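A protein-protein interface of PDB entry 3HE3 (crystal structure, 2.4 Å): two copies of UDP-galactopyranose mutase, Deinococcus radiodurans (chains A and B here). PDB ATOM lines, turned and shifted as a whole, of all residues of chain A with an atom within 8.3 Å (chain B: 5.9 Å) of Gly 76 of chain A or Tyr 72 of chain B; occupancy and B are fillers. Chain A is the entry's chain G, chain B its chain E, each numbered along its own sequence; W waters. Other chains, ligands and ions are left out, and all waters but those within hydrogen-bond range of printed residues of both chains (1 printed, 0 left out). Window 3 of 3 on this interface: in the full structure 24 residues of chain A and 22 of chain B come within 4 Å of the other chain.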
ATOM      1  N   CYS A  71       0.722 -10.107   9.379  1.00  0.00           N
ATOM      2  CA  CYS A  71      -0.406 -10.761  10.024  1.00  0.00           C
ATOM      3  C   CYS A  71      -1.627 -10.676   9.121  1.00  0.00           C
ATOM      4  O   CYS A  71      -1.590 -10.031   8.075  1.00  0.00           O
ATOM      5  CB  CYS A  71      -0.701 -10.096  11.365  1.00  0.00           C
ATOM      6  SG  CYS A  71      -1.137  -8.346  11.243  1.00  0.00           S
ATOM      7  N   TYR A  72      -2.710 -11.331   9.523  1.00  0.00           N
ATOM      8  CA  TYR A  72      -3.949 -11.284   8.756  1.00  0.00           C
ATOM      9  C   TYR A  72      -4.914 -10.258   9.339  1.00  0.00           C
ATOM     10  O   TYR A  72      -5.169 -10.245  10.543  1.00  0.00           O
ATOM     11  CB  TYR A  72      -4.606 -12.664   8.700  1.00  0.00           C
ATOM     12  CG  TYR A  72      -3.916 -13.632   7.765  1.00  0.00           C
ATOM     13  CD1 TYR A  72      -4.400 -13.852   6.482  1.00  0.00           C
ATOM     14  CD2 TYR A  72      -2.778 -14.321   8.162  1.00  0.00           C
ATOM     15  CE1 TYR A  72      -3.773 -14.736   5.623  1.00  0.00           C
ATOM     16  CE2 TYR A  72      -2.141 -15.206   7.306  1.00  0.00           C
ATOM     17  CZ  TYR A  72      -2.644 -15.409   6.041  1.00  0.00           C
ATOM     18  OH  TYR A  72      -2.019 -16.288   5.191  1.00  0.00           O
ATOM     19  N   ASP A  73      -5.445  -9.396   8.479  1.00  0.00           N
ATOM     20  CA  ASP A  73      -6.396  -8.376   8.915  1.00  0.00           C
ATOM     21  C   ASP A  73      -7.808  -8.945   9.032  1.00  0.00           C
ATOM     22  O   ASP A  73      -8.034 -10.133   8.774  1.00  0.00           O
ATOM     23  CB  ASP A  73      -6.367  -7.157   7.983  1.00  0.00           C
ATOM     24  CG  ASP A  73      -6.851  -7.472   6.579  1.00  0.00           C
ATOM     25  OD1 ASP A  73      -7.506  -8.517   6.374  1.00  0.00           O
ATOM     26  OD2 ASP A  73      -6.585  -6.655   5.674  1.00  0.00           O
ATOM     27  N   ASP A  74      -8.753  -8.097   9.425  1.00  0.00           N
ATOM     28  CA  ASP A  74     -10.122  -8.540   9.664  1.00  0.00           C
ATOM     29  C   ASP A  74     -10.749  -9.199   8.437  1.00  0.00           C
ATOM     30  O   ASP A  74     -11.642 -10.033   8.569  1.00  0.00           O
ATOM     31  CB  ASP A  74     -10.986  -7.374  10.150  1.00  0.00           C
ATOM     32  CG  ASP A  74     -10.512  -6.813  11.481  1.00  0.00           C
ATOM     33  OD1 ASP A  74      -9.702  -7.485  12.156  1.00  0.00           O
ATOM     34  OD2 ASP A  74     -10.946  -5.702  11.854  1.00  0.00           O
ATOM     35  N   ALA A  75     -10.273  -8.834   7.250  1.00  0.00           N
ATOM     36  CA  ALA A  75     -10.829  -9.374   6.012  1.00  0.00           C
ATOM     37  C   ALA A  75     -10.174 -10.693   5.610  1.00  0.00           C
ATOM     38  O   ALA A  75     -10.641 -11.368   4.698  1.00  0.00           O
ATOM     39  CB  ALA A  75     -10.718  -8.357   4.878  1.00  0.00           C
ATOM     40  N   GLY A  76      -9.096 -11.058   6.295  1.00  0.00           N
ATOM     41  CA  GLY A  76      -8.387 -12.287   5.987  1.00  0.00           C
ATOM     42  C   GLY A  76      -7.311 -12.070   4.939  1.00  0.00           C
ATOM     43  O   GLY A  76      -6.893 -13.001   4.252  1.00  0.00           O
ATOM     44  N   VAL A  77      -6.870 -10.824   4.815  1.00  0.00           N
ATOM     45  CA  VAL A  77      -5.821 -10.467   3.872  1.00  0.00           C
ATOM     46  C   VAL A  77      -4.488 -10.305   4.604  1.00  0.00           C
ATOM     47  O   VAL A  77      -4.418  -9.643   5.636  1.00  0.00           O
ATOM     48  CB  VAL A  77      -6.176  -9.173   3.111  1.00  0.00           C
ATOM     49  CG1 VAL A  77      -4.979  -8.666   2.322  1.00  0.00           C
ATOM     50  CG2 VAL A  77      -7.361  -9.415   2.184  1.00  0.00           C
ATOM     51  N   LEU A  78      -3.437 -10.923   4.073  1.00  0.00           N
ATOM     52  CA  LEU A  78      -2.111 -10.860   4.685  1.00  0.00           C
ATOM     53  C   LEU A  78      -1.429  -9.526   4.404  1.00  0.00           C
ATOM     54  O   LEU A  78      -1.069  -9.230   3.270  1.00  0.00           O
ATOM     55  CB  LEU A  78      -1.236 -12.015   4.198  1.00  0.00           C
ATOM     56  CG  LEU A  78       0.217 -11.993   4.680  1.00  0.00           C
ATOM     57  CD1 LEU A  78       0.270 -12.015   6.200  1.00  0.00           C
ATOM     58  CD2 LEU A  78       1.002 -13.160   4.089  1.00  0.00           C
ATOM     59  N   ILE A  79      -1.240  -8.732   5.452  1.00  0.00           N
ATOM     60  CA  ILE A  79      -0.697  -7.390   5.308  1.00  0.00           C
ATOM     61  C   ILE A  79       0.536  -7.195   6.178  1.00  0.00           C
ATOM     62  O   ILE A  79       0.854  -8.037   7.014  1.00  0.00           O
ATOM     63  CB  ILE A  79      -1.735  -6.343   5.725  1.00  0.00           C
ATOM     64  CG1 ILE A  79      -2.112  -6.538   7.196  1.00  0.00           C
ATOM     65  CG2 ILE A  79      -2.969  -6.449   4.846  1.00  0.00           C
ATOM     66  CD1 ILE A  79      -2.883  -5.384   7.791  1.00  0.00           C
ATOM     67  N   HIS A 220       5.151 -17.801   3.265  1.00  0.00           N
ATOM     68  CA  HIS A 220       4.034 -17.688   4.200  1.00  0.00           C
ATOM     69  C   HIS A 220       4.127 -16.461   5.092  1.00  0.00           C
ATOM     70  O   HIS A 220       3.522 -16.415   6.161  1.00  0.00           O
ATOM     71  CB  HIS A 220       3.933 -18.942   5.068  1.00  0.00           C
ATOM     72  CG  HIS A 220       3.706 -20.197   4.286  1.00  0.00           C
ATOM     73  ND1 HIS A 220       2.516 -20.467   3.644  1.00  0.00           N
ATOM     74  CD2 HIS A 220       4.517 -21.251   4.036  1.00  0.00           C
ATOM     75  CE1 HIS A 220       2.604 -21.636   3.034  1.00  0.00           C
ATOM     76  NE2 HIS A 220       3.807 -22.132   3.257  1.00  0.00           N
ATOM     77  N   ARG A 224       5.823 -16.178  10.156  1.00  0.00           N
ATOM     78  CA  ARG A 224       6.036 -17.620  10.118  1.00  0.00           C
ATOM     79  C   ARG A 224       7.521 -17.949  10.078  1.00  0.00           C
ATOM     80  O   ARG A 224       7.978 -18.900  10.716  1.00  0.00           O
ATOM     81  CB  ARG A 224       5.335 -18.233   8.911  1.00  0.00           C
ATOM     82  CG  ARG A 224       3.827 -18.334   9.075  1.00  0.00           C
ATOM     83  CD  ARG A 224       3.453 -19.522   9.950  1.00  0.00           C
ATOM     84  NE  ARG A 224       3.871 -20.779   9.341  1.00  0.00           N
ATOM     85  CZ  ARG A 224       3.176 -21.421   8.407  1.00  0.00           C
ATOM     86  NH1 ARG A 224       2.024 -20.919   7.977  1.00  0.00           N
ATOM     87  NH2 ARG A 224       3.632 -22.560   7.902  1.00  0.00           N
ATOM     88  N   GLN A 227       9.094 -17.262  13.442  1.00  0.00           N
ATOM     89  CA  GLN A 227       8.704 -18.298  14.382  1.00  0.00           C
ATOM     90  C   GLN A 227       9.650 -19.488  14.306  1.00  0.00           C
ATOM     91  O   GLN A 227       9.972 -20.102  15.322  1.00  0.00           O
ATOM     92  CB  GLN A 227       7.261 -18.737  14.136  1.00  0.00           C
ATOM     93  CG  GLN A 227       6.237 -17.708  14.579  1.00  0.00           C
ATOM     94  CD  GLN A 227       4.822 -18.087  14.191  1.00  0.00           C
ATOM     95  OE1 GLN A 227       4.593 -19.094  13.520  1.00  0.00           O
ATOM     96  NE2 GLN A 227       3.861 -17.276  14.616  1.00  0.00           N
ATOM     97  N   THR A 283      -9.424  -1.695   3.380  1.00  0.00           N
ATOM     98  CA  THR A 283      -9.828  -2.877   2.632  1.00  0.00           C
ATOM     99  C   THR A 283     -10.899  -2.465   1.626  1.00  0.00           C
ATOM    100  O   THR A 283     -11.784  -1.681   1.949  1.00  0.00           O
ATOM    101  CB  THR A 283     -10.370  -3.983   3.567  1.00  0.00           C
ATOM    102  OG1 THR A 283      -9.338  -4.391   4.476  1.00  0.00           O
ATOM    103  CG2 THR A 283     -10.836  -5.190   2.769  1.00  0.00           C
ATOM    104  N   LYS A 310      -1.429  -7.674  -1.897  1.00  0.00           N
ATOM    105  CA  LYS A 310      -1.614  -8.873  -2.719  1.00  0.00           C
ATOM    106  C   LYS A 310      -0.583  -8.997  -3.844  1.00  0.00           C
ATOM    107  O   LYS A 310      -0.211 -10.107  -4.224  1.00  0.00           O
ATOM    108  CB  LYS A 310      -3.043  -8.975  -3.256  1.00  0.00           C
ATOM    109  CG  LYS A 310      -4.053  -9.366  -2.188  1.00  0.00           C
ATOM    110  CD  LYS A 310      -5.484  -9.161  -2.658  1.00  0.00           C
ATOM    111  CE  LYS A 310      -5.876 -10.182  -3.707  1.00  0.00           C
ATOM    112  NZ  LYS A 310      -7.234  -9.905  -4.251  1.00  0.00           N
ATOM    113  N   GLN A 315      -1.140 -13.583  -2.502  1.00  0.00           N
ATOM    114  CA  GLN A 315      -2.354 -14.158  -1.937  1.00  0.00           C
ATOM    115  C   GLN A 315      -3.531 -14.032  -2.900  1.00  0.00           C
ATOM    116  O   GLN A 315      -3.604 -13.091  -3.686  1.00  0.00           O
ATOM    117  CB  GLN A 315      -2.693 -13.483  -0.605  1.00  0.00           C
ATOM    118  CG  GLN A 315      -3.918 -14.056   0.087  1.00  0.00           C
ATOM    119  CD  GLN A 315      -4.289 -13.286   1.335  1.00  0.00           C
ATOM    120  OE1 GLN A 315      -3.774 -12.196   1.576  1.00  0.00           O
ATOM    121  NE2 GLN A 315      -5.187 -13.848   2.136  1.00  0.00           N
ATOM    122  N   ARG A 316      -4.447 -14.990  -2.826  1.00  0.00           N
ATOM    123  CA  ARG A 316      -5.661 -14.959  -3.627  1.00  0.00           C
ATOM    124  C   ARG A 316      -6.831 -14.627  -2.720  1.00  0.00           C
ATOM    125  O   ARG A 316      -7.095 -15.346  -1.760  1.00  0.00           O
ATOM    126  CB  ARG A 316      -5.897 -16.317  -4.278  1.00  0.00           C
ATOM    127  CG  ARG A 316      -6.462 -16.240  -5.678  1.00  0.00           C
ATOM    128  CD  ARG A 316      -7.093 -17.552  -6.093  1.00  0.00           C
ATOM    129  NE  ARG A 316      -8.549 -17.492  -6.029  1.00  0.00           N
ATOM    130  CZ  ARG A 316      -9.353 -18.400  -6.571  1.00  0.00           C
ATOM    131  NH1 ARG A 316      -8.836 -19.442  -7.207  1.00  0.00           N
ATOM    132  NH2 ARG A 316     -10.671 -18.268  -6.476  1.00  0.00           N
ATOM    133  N   HIS A 317      -7.535 -13.541  -3.018  1.00  0.00           N
ATOM    134  CA  HIS A 317      -8.604 -13.072  -2.145  1.00  0.00           C
ATOM    135  C   HIS A 317      -9.634 -12.285  -2.954  1.00  0.00           C
ATOM    136  O   HIS A 317      -9.285 -11.630  -3.937  1.00  0.00           O
ATOM    137  CB  HIS A 317      -8.015 -12.201  -1.032  1.00  0.00           C
ATOM    138  CG  HIS A 317      -8.846 -12.159   0.211  1.00  0.00           C
ATOM    139  ND1 HIS A 317      -9.870 -11.257   0.395  1.00  0.00           N
ATOM    140  CD2 HIS A 317      -8.795 -12.904   1.341  1.00  0.00           C
ATOM    141  CE1 HIS A 317     -10.418 -11.447   1.579  1.00  0.00           C
ATOM    142  NE2 HIS A 317      -9.784 -12.442   2.177  1.00  0.00           N
ATOM    143  N   HIS A 318     -10.901 -12.352  -2.548  1.00  0.00           N
ATOM    144  CA  HIS A 318     -11.960 -11.657  -3.277  1.00  0.00           C
ATOM    145  C   HIS A 318     -11.957 -10.163  -2.978  1.00  0.00           C
ATOM    146  O   HIS A 318     -12.650  -9.382  -3.634  1.00  0.00           O
ATOM    147  CB  HIS A 318     -13.334 -12.269  -2.990  1.00  0.00           C
ATOM    148  CG  HIS A 318     -13.677 -12.345  -1.536  1.00  0.00           C
ATOM    149  ND1 HIS A 318     -13.057 -13.223  -0.671  1.00  0.00           N
ATOM    150  CD2 HIS A 318     -14.585 -11.667  -0.797  1.00  0.00           C
ATOM    151  CE1 HIS A 318     -13.565 -13.075   0.542  1.00  0.00           C
ATOM    152  NE2 HIS A 318     -14.494 -12.137   0.492  1.00  0.00           N
ATOM    153  N   GLN A 319     -11.168  -9.774  -1.983  1.00  0.00           N
ATOM    154  CA  GLN A 319     -11.027  -8.376  -1.618  1.00  0.00           C
ATOM    155  C   GLN A 319      -9.560  -7.972  -1.644  1.00  0.00           C
ATOM    156  O   GLN A 319      -8.703  -8.753  -2.051  1.00  0.00           O
ATOM    157  CB  GLN A 319     -11.634  -8.130  -0.239  1.00  0.00           C
ATOM    158  CG  GLN A 319     -13.134  -8.378  -0.196  1.00  0.00           C
ATOM    159  CD  GLN A 319     -13.740  -8.083   1.158  1.00  0.00           C
ATOM    160  OE1 GLN A 319     -13.169  -8.420   2.195  1.00  0.00           O
ATOM    161  NE2 GLN A 319     -14.912  -7.457   1.156  1.00  0.00           N
ATOM    162  N   SER A 321      -6.423  -5.278   0.422  1.00  0.00           N
ATOM    163  CA  SER A 321      -6.046  -4.345   1.476  1.00  0.00           C
ATOM    164  C   SER A 321      -4.846  -3.510   1.065  1.00  0.00           C
ATOM    165  O   SER A 321      -3.851  -4.035   0.579  1.00  0.00           O
ATOM    166  CB  SER A 321      -5.743  -5.089   2.780  1.00  0.00           C
ATOM    167  OG  SER A 321      -6.919  -5.658   3.324  1.00  0.00           O
ATOM    168  N   ASP B  70      -6.125 -20.117  17.861  1.00  0.00           N
ATOM    169  CA  ASP B  70      -6.302 -20.281  16.420  1.00  0.00           C
ATOM    170  C   ASP B  70      -5.305 -19.476  15.597  1.00  0.00           C
ATOM    171  O   ASP B  70      -4.638 -18.570  16.100  1.00  0.00           O
ATOM    172  CB  ASP B  70      -7.751 -20.049  15.947  1.00  0.00           C
ATOM    173  CG  ASP B  70      -8.322 -18.717  16.388  1.00  0.00           C
ATOM    174  OD1 ASP B  70      -9.568 -18.625  16.481  1.00  0.00           O
ATOM    175  OD2 ASP B  70      -7.549 -17.766  16.631  1.00  0.00           O
ATOM    176  N   CYS B  71      -5.191 -19.849  14.330  1.00  0.00           N
ATOM    177  CA  CYS B  71      -4.239 -19.221  13.438  1.00  0.00           C
ATOM    178  C   CYS B  71      -4.575 -19.575  12.004  1.00  0.00           C
ATOM    179  O   CYS B  71      -5.387 -20.466  11.743  1.00  0.00           O
ATOM    180  CB  CYS B  71      -2.818 -19.684  13.758  1.00  0.00           C
ATOM    181  SG  CYS B  71      -2.534 -21.452  13.490  1.00  0.00           S
ATOM    182  N   TYR B  72      -3.938 -18.866  11.083  1.00  0.00           N
ATOM    183  CA  TYR B  72      -4.116 -19.104   9.665  1.00  0.00           C
ATOM    184  C   TYR B  72      -3.112 -20.144   9.175  1.00  0.00           C
ATOM    185  O   TYR B  72      -1.916 -20.044   9.459  1.00  0.00           O
ATOM    186  CB  TYR B  72      -3.960 -17.789   8.900  1.00  0.00           C
ATOM    187  CG  TYR B  72      -5.183 -16.907   9.003  1.00  0.00           C
ATOM    188  CD1 TYR B  72      -6.145 -16.913   8.006  1.00  0.00           C
ATOM    189  CD2 TYR B  72      -5.384 -16.083  10.105  1.00  0.00           C
ATOM    190  CE1 TYR B  72      -7.268 -16.121   8.091  1.00  0.00           C
ATOM    191  CE2 TYR B  72      -6.512 -15.284  10.202  1.00  0.00           C
ATOM    192  CZ  TYR B  72      -7.452 -15.310   9.189  1.00  0.00           C
ATOM    193  OH  TYR B  72      -8.582 -14.520   9.261  1.00  0.00           O
ATOM    194  N   ASP B  73      -3.604 -21.147   8.448  1.00  0.00           N
ATOM    195  CA  ASP B  73      -2.736 -22.190   7.910  1.00  0.00           C
ATOM    196  C   ASP B  73      -2.069 -21.756   6.605  1.00  0.00           C
ATOM    197  O   ASP B  73      -2.215 -20.612   6.175  1.00  0.00           O
ATOM    198  CB  ASP B  73      -3.497 -23.511   7.729  1.00  0.00           C
ATOM    199  CG  ASP B  73      -4.637 -23.406   6.733  1.00  0.00           C
ATOM    200  OD1 ASP B  73      -4.730 -22.381   6.017  1.00  0.00           O
ATOM    201  OD2 ASP B  73      -5.443 -24.360   6.664  1.00  0.00           O
ATOM    202  N   ASP B  74      -1.329 -22.673   5.990  1.00  0.00           N
ATOM    203  CA  ASP B  74      -0.583 -22.378   4.767  1.00  0.00           C
ATOM    204  C   ASP B  74      -1.466 -21.866   3.629  1.00  0.00           C
ATOM    205  O   ASP B  74      -1.001 -21.111   2.774  1.00  0.00           O
ATOM    206  CB  ASP B  74       0.189 -23.616   4.294  1.00  0.00           C
ATOM    207  CG  ASP B  74       1.336 -23.978   5.214  1.00  0.00           C
ATOM    208  OD1 ASP B  74       1.660 -23.175   6.112  1.00  0.00           O
ATOM    209  OD2 ASP B  74       1.919 -25.067   5.036  1.00  0.00           O
ATOM    210  N   GLY B  76      -4.239 -20.066   3.959  1.00  0.00           N
ATOM    211  CA  GLY B  76      -4.914 -18.826   4.294  1.00  0.00           C
ATOM    212  C   GLY B  76      -6.278 -19.048   4.919  1.00  0.00           C
ATOM    213  O   GLY B  76      -7.116 -18.146   4.944  1.00  0.00           O
ATOM    214  N   VAL B  77      -6.501 -20.258   5.421  1.00  0.00           N
ATOM    215  CA  VAL B  77      -7.742 -20.580   6.114  1.00  0.00           C
ATOM    216  C   VAL B  77      -7.530 -20.509   7.624  1.00  0.00           C
ATOM    217  O   VAL B  77      -6.457 -20.863   8.125  1.00  0.00           O
ATOM    218  CB  VAL B  77      -8.261 -21.978   5.730  1.00  0.00           C
ATOM    219  CG1 VAL B  77      -9.587 -22.277   6.435  1.00  0.00           C
ATOM    220  CG2 VAL B  77      -8.407 -22.085   4.225  1.00  0.00           C
ATOM    221  N   LEU B  78      -8.549 -20.039   8.340  1.00  0.00           N
ATOM    222  CA  LEU B  78      -8.489 -19.910   9.793  1.00  0.00           C
ATOM    223  C   LEU B  78      -8.886 -21.226  10.459  1.00  0.00           C
ATOM    224  O   LEU B  78      -9.990 -21.720  10.243  1.00  0.00           O
ATOM    225  CB  LEU B  78      -9.410 -18.779  10.255  1.00  0.00           C
ATOM    226  CG  LEU B  78      -9.517 -18.525  11.756  1.00  0.00           C
ATOM    227  CD1 LEU B  78      -8.132 -18.454  12.379  1.00  0.00           C
ATOM    228  CD2 LEU B  78     -10.292 -17.243  12.009  1.00  0.00           C
ATOM    229  N   ILE B  79      -7.990 -21.787  11.267  1.00  0.00           N
ATOM    230  CA  ILE B  79      -8.212 -23.112  11.850  1.00  0.00           C
ATOM    231  C   ILE B  79      -7.882 -23.171  13.335  1.00  0.00           C
ATOM    232  O   ILE B  79      -7.337 -22.225  13.898  1.00  0.00           O
ATOM    233  CB  ILE B  79      -7.336 -24.163  11.162  1.00  0.00           C
ATOM    234  CG1 ILE B  79      -5.859 -23.821  11.374  1.00  0.00           C
ATOM    235  CG2 ILE B  79      -7.672 -24.255   9.681  1.00  0.00           C
ATOM    236  CD1 ILE B  79      -4.935 -24.998  11.259  1.00  0.00           C
ATOM    237  N   HIS B 220     -13.051 -12.524  15.089  1.00  0.00           N
ATOM    238  CA  HIS B 220     -11.757 -12.638  14.427  1.00  0.00           C
ATOM    239  C   HIS B 220     -10.867 -13.711  15.046  1.00  0.00           C
ATOM    240  O   HIS B 220      -9.642 -13.660  14.913  1.00  0.00           O
ATOM    241  CB  HIS B 220     -11.030 -11.292  14.426  1.00  0.00           C
ATOM    242  CG  HIS B 220     -11.867 -10.156  13.933  1.00  0.00           C
ATOM    243  ND1 HIS B 220     -12.338 -10.083  12.638  1.00  0.00           N
ATOM    244  CD2 HIS B 220     -12.319  -9.043  14.556  1.00  0.00           C
ATOM    245  CE1 HIS B 220     -13.044  -8.980  12.488  1.00  0.00           C
ATOM    246  NE2 HIS B 220     -13.049  -8.327  13.637  1.00  0.00           N
ATOM    247  N   GLN B 315     -15.758 -18.018   7.535  1.00  0.00           N
ATOM    248  CA  GLN B 315     -14.794 -17.496   6.574  1.00  0.00           C
ATOM    249  C   GLN B 315     -15.159 -17.868   5.140  1.00  0.00           C
ATOM    250  O   GLN B 315     -15.718 -18.931   4.876  1.00  0.00           O
ATOM    251  CB  GLN B 315     -13.372 -17.980   6.890  1.00  0.00           C
ATOM    252  CG  GLN B 315     -12.310 -17.422   5.942  1.00  0.00           C
ATOM    253  CD  GLN B 315     -10.907 -17.918   6.254  1.00  0.00           C
ATOM    254  OE1 GLN B 315     -10.732 -18.969   6.868  1.00  0.00           O
ATOM    255  NE2 GLN B 315      -9.902 -17.161   5.827  1.00  0.00           N
HETATM  256  O   HOH W   1      -7.482 -15.604   3.848  1.00  0.00           O
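OD1 of Asp 74 of chain B lies within salt-bridge range of NH2 of Arg 224 of chain A.
Printed residues of chain B within 4 Å of Tyr 72 of chain A: Tyr 72 and Gly 76.
Of the printed residues of chain B, Asp 74 of chain A touches His 220 (3.5 Å).
Of chain B, only Tyr 72 comes within 4 Å of Gly 76 of chain A.
Tyr 72 of chain B touches just these residues of chain A: Tyr 72 (3.5 Å) and Gly 76 (3.97 Å).
Of the printed residues of chain A, Gly 76 of chain B touches Tyr 72.
Of the printed residues of chain A, His 220 of chain B touches Asp 74 (3.5 Å).
The nearest residue of chain B that does not touch Gly 76 of chain A is Gln 315 of chain B (5.1 Å).
The nearest residue of chain A that does not touch Tyr 72 of chain B is Arg 224 of chain A (4.3 Å).
OD1 of Asp 73 of chain B lies within hydrogen-bond range of N of Gly 76 of chain B.
The side-chain amide nitrogen (NE2) of Gln 315 of chain B lies within hydrogen-bond range of the backbone carbonyl oxygen (O) of Gly 76 of chain B (3.1 Å).
N of Gly 76 of chain A lies within hydrogen-bond range of OD1 of Asp 73 of chain A (3.0 Å).
O of Gly 76 of chain A sits at hydrogen-bond distance from NE2 of Gln 315 of chain A (2.8 Å).
Tyr 72 of chain B touches its own counterpart, Tyr 72 of chain A.
Tyr 72 of chain A touches Gly 76 of chain B, and with the chains exchanged Gly 76 of chain A touches Tyr 72 of chain B.
Asp 74 of chain A touches His 220 of chain B, and with the chains exchanged His 220 of chain A touches Asp 74 of chain B.
Positions printed for both chains: 71, 72, 73, 74, 76, 77, 78, 79, 220 and 315.
Hydrophobic or aromatic side chains of chain A that line the printed part of chain B: Tyr 72 and His 220.
Among the printed residues, 6 pairs touch across the chains.
Among the printed residues, Asp or Glu carboxylates within 4 Å of a Lys or Arg side-chain nitrogen of the other chain: Arg 224 of chain A with Asp 74 of chain B (2.7 Å).
Water W1 lies within hydrogen-bond range of the backbone carbonyl oxygen of Gly 76 of chain A, the backbone carbonyl oxygen of Gly 76 of chain B, the side-chain amide nitrogen of Gln 315 of chain A and the side-chain amide nitrogen of Gln 315 of chain B.
Tyr 72 of chain B touches Tyr 72 of chain A.
Gly 76 of chain B touches Tyr 72 of chain A.
CG of Asp 74 of chain A touches CE1 of His 220 of chain B, 3.5 Å away.
Gly 76 of chain A touches Tyr 72 of chain B (CA to OH, 3.97 Å).
His 220 of chain A touches Asp 74 of chain B (CE1 to CB, 3.4 Å).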
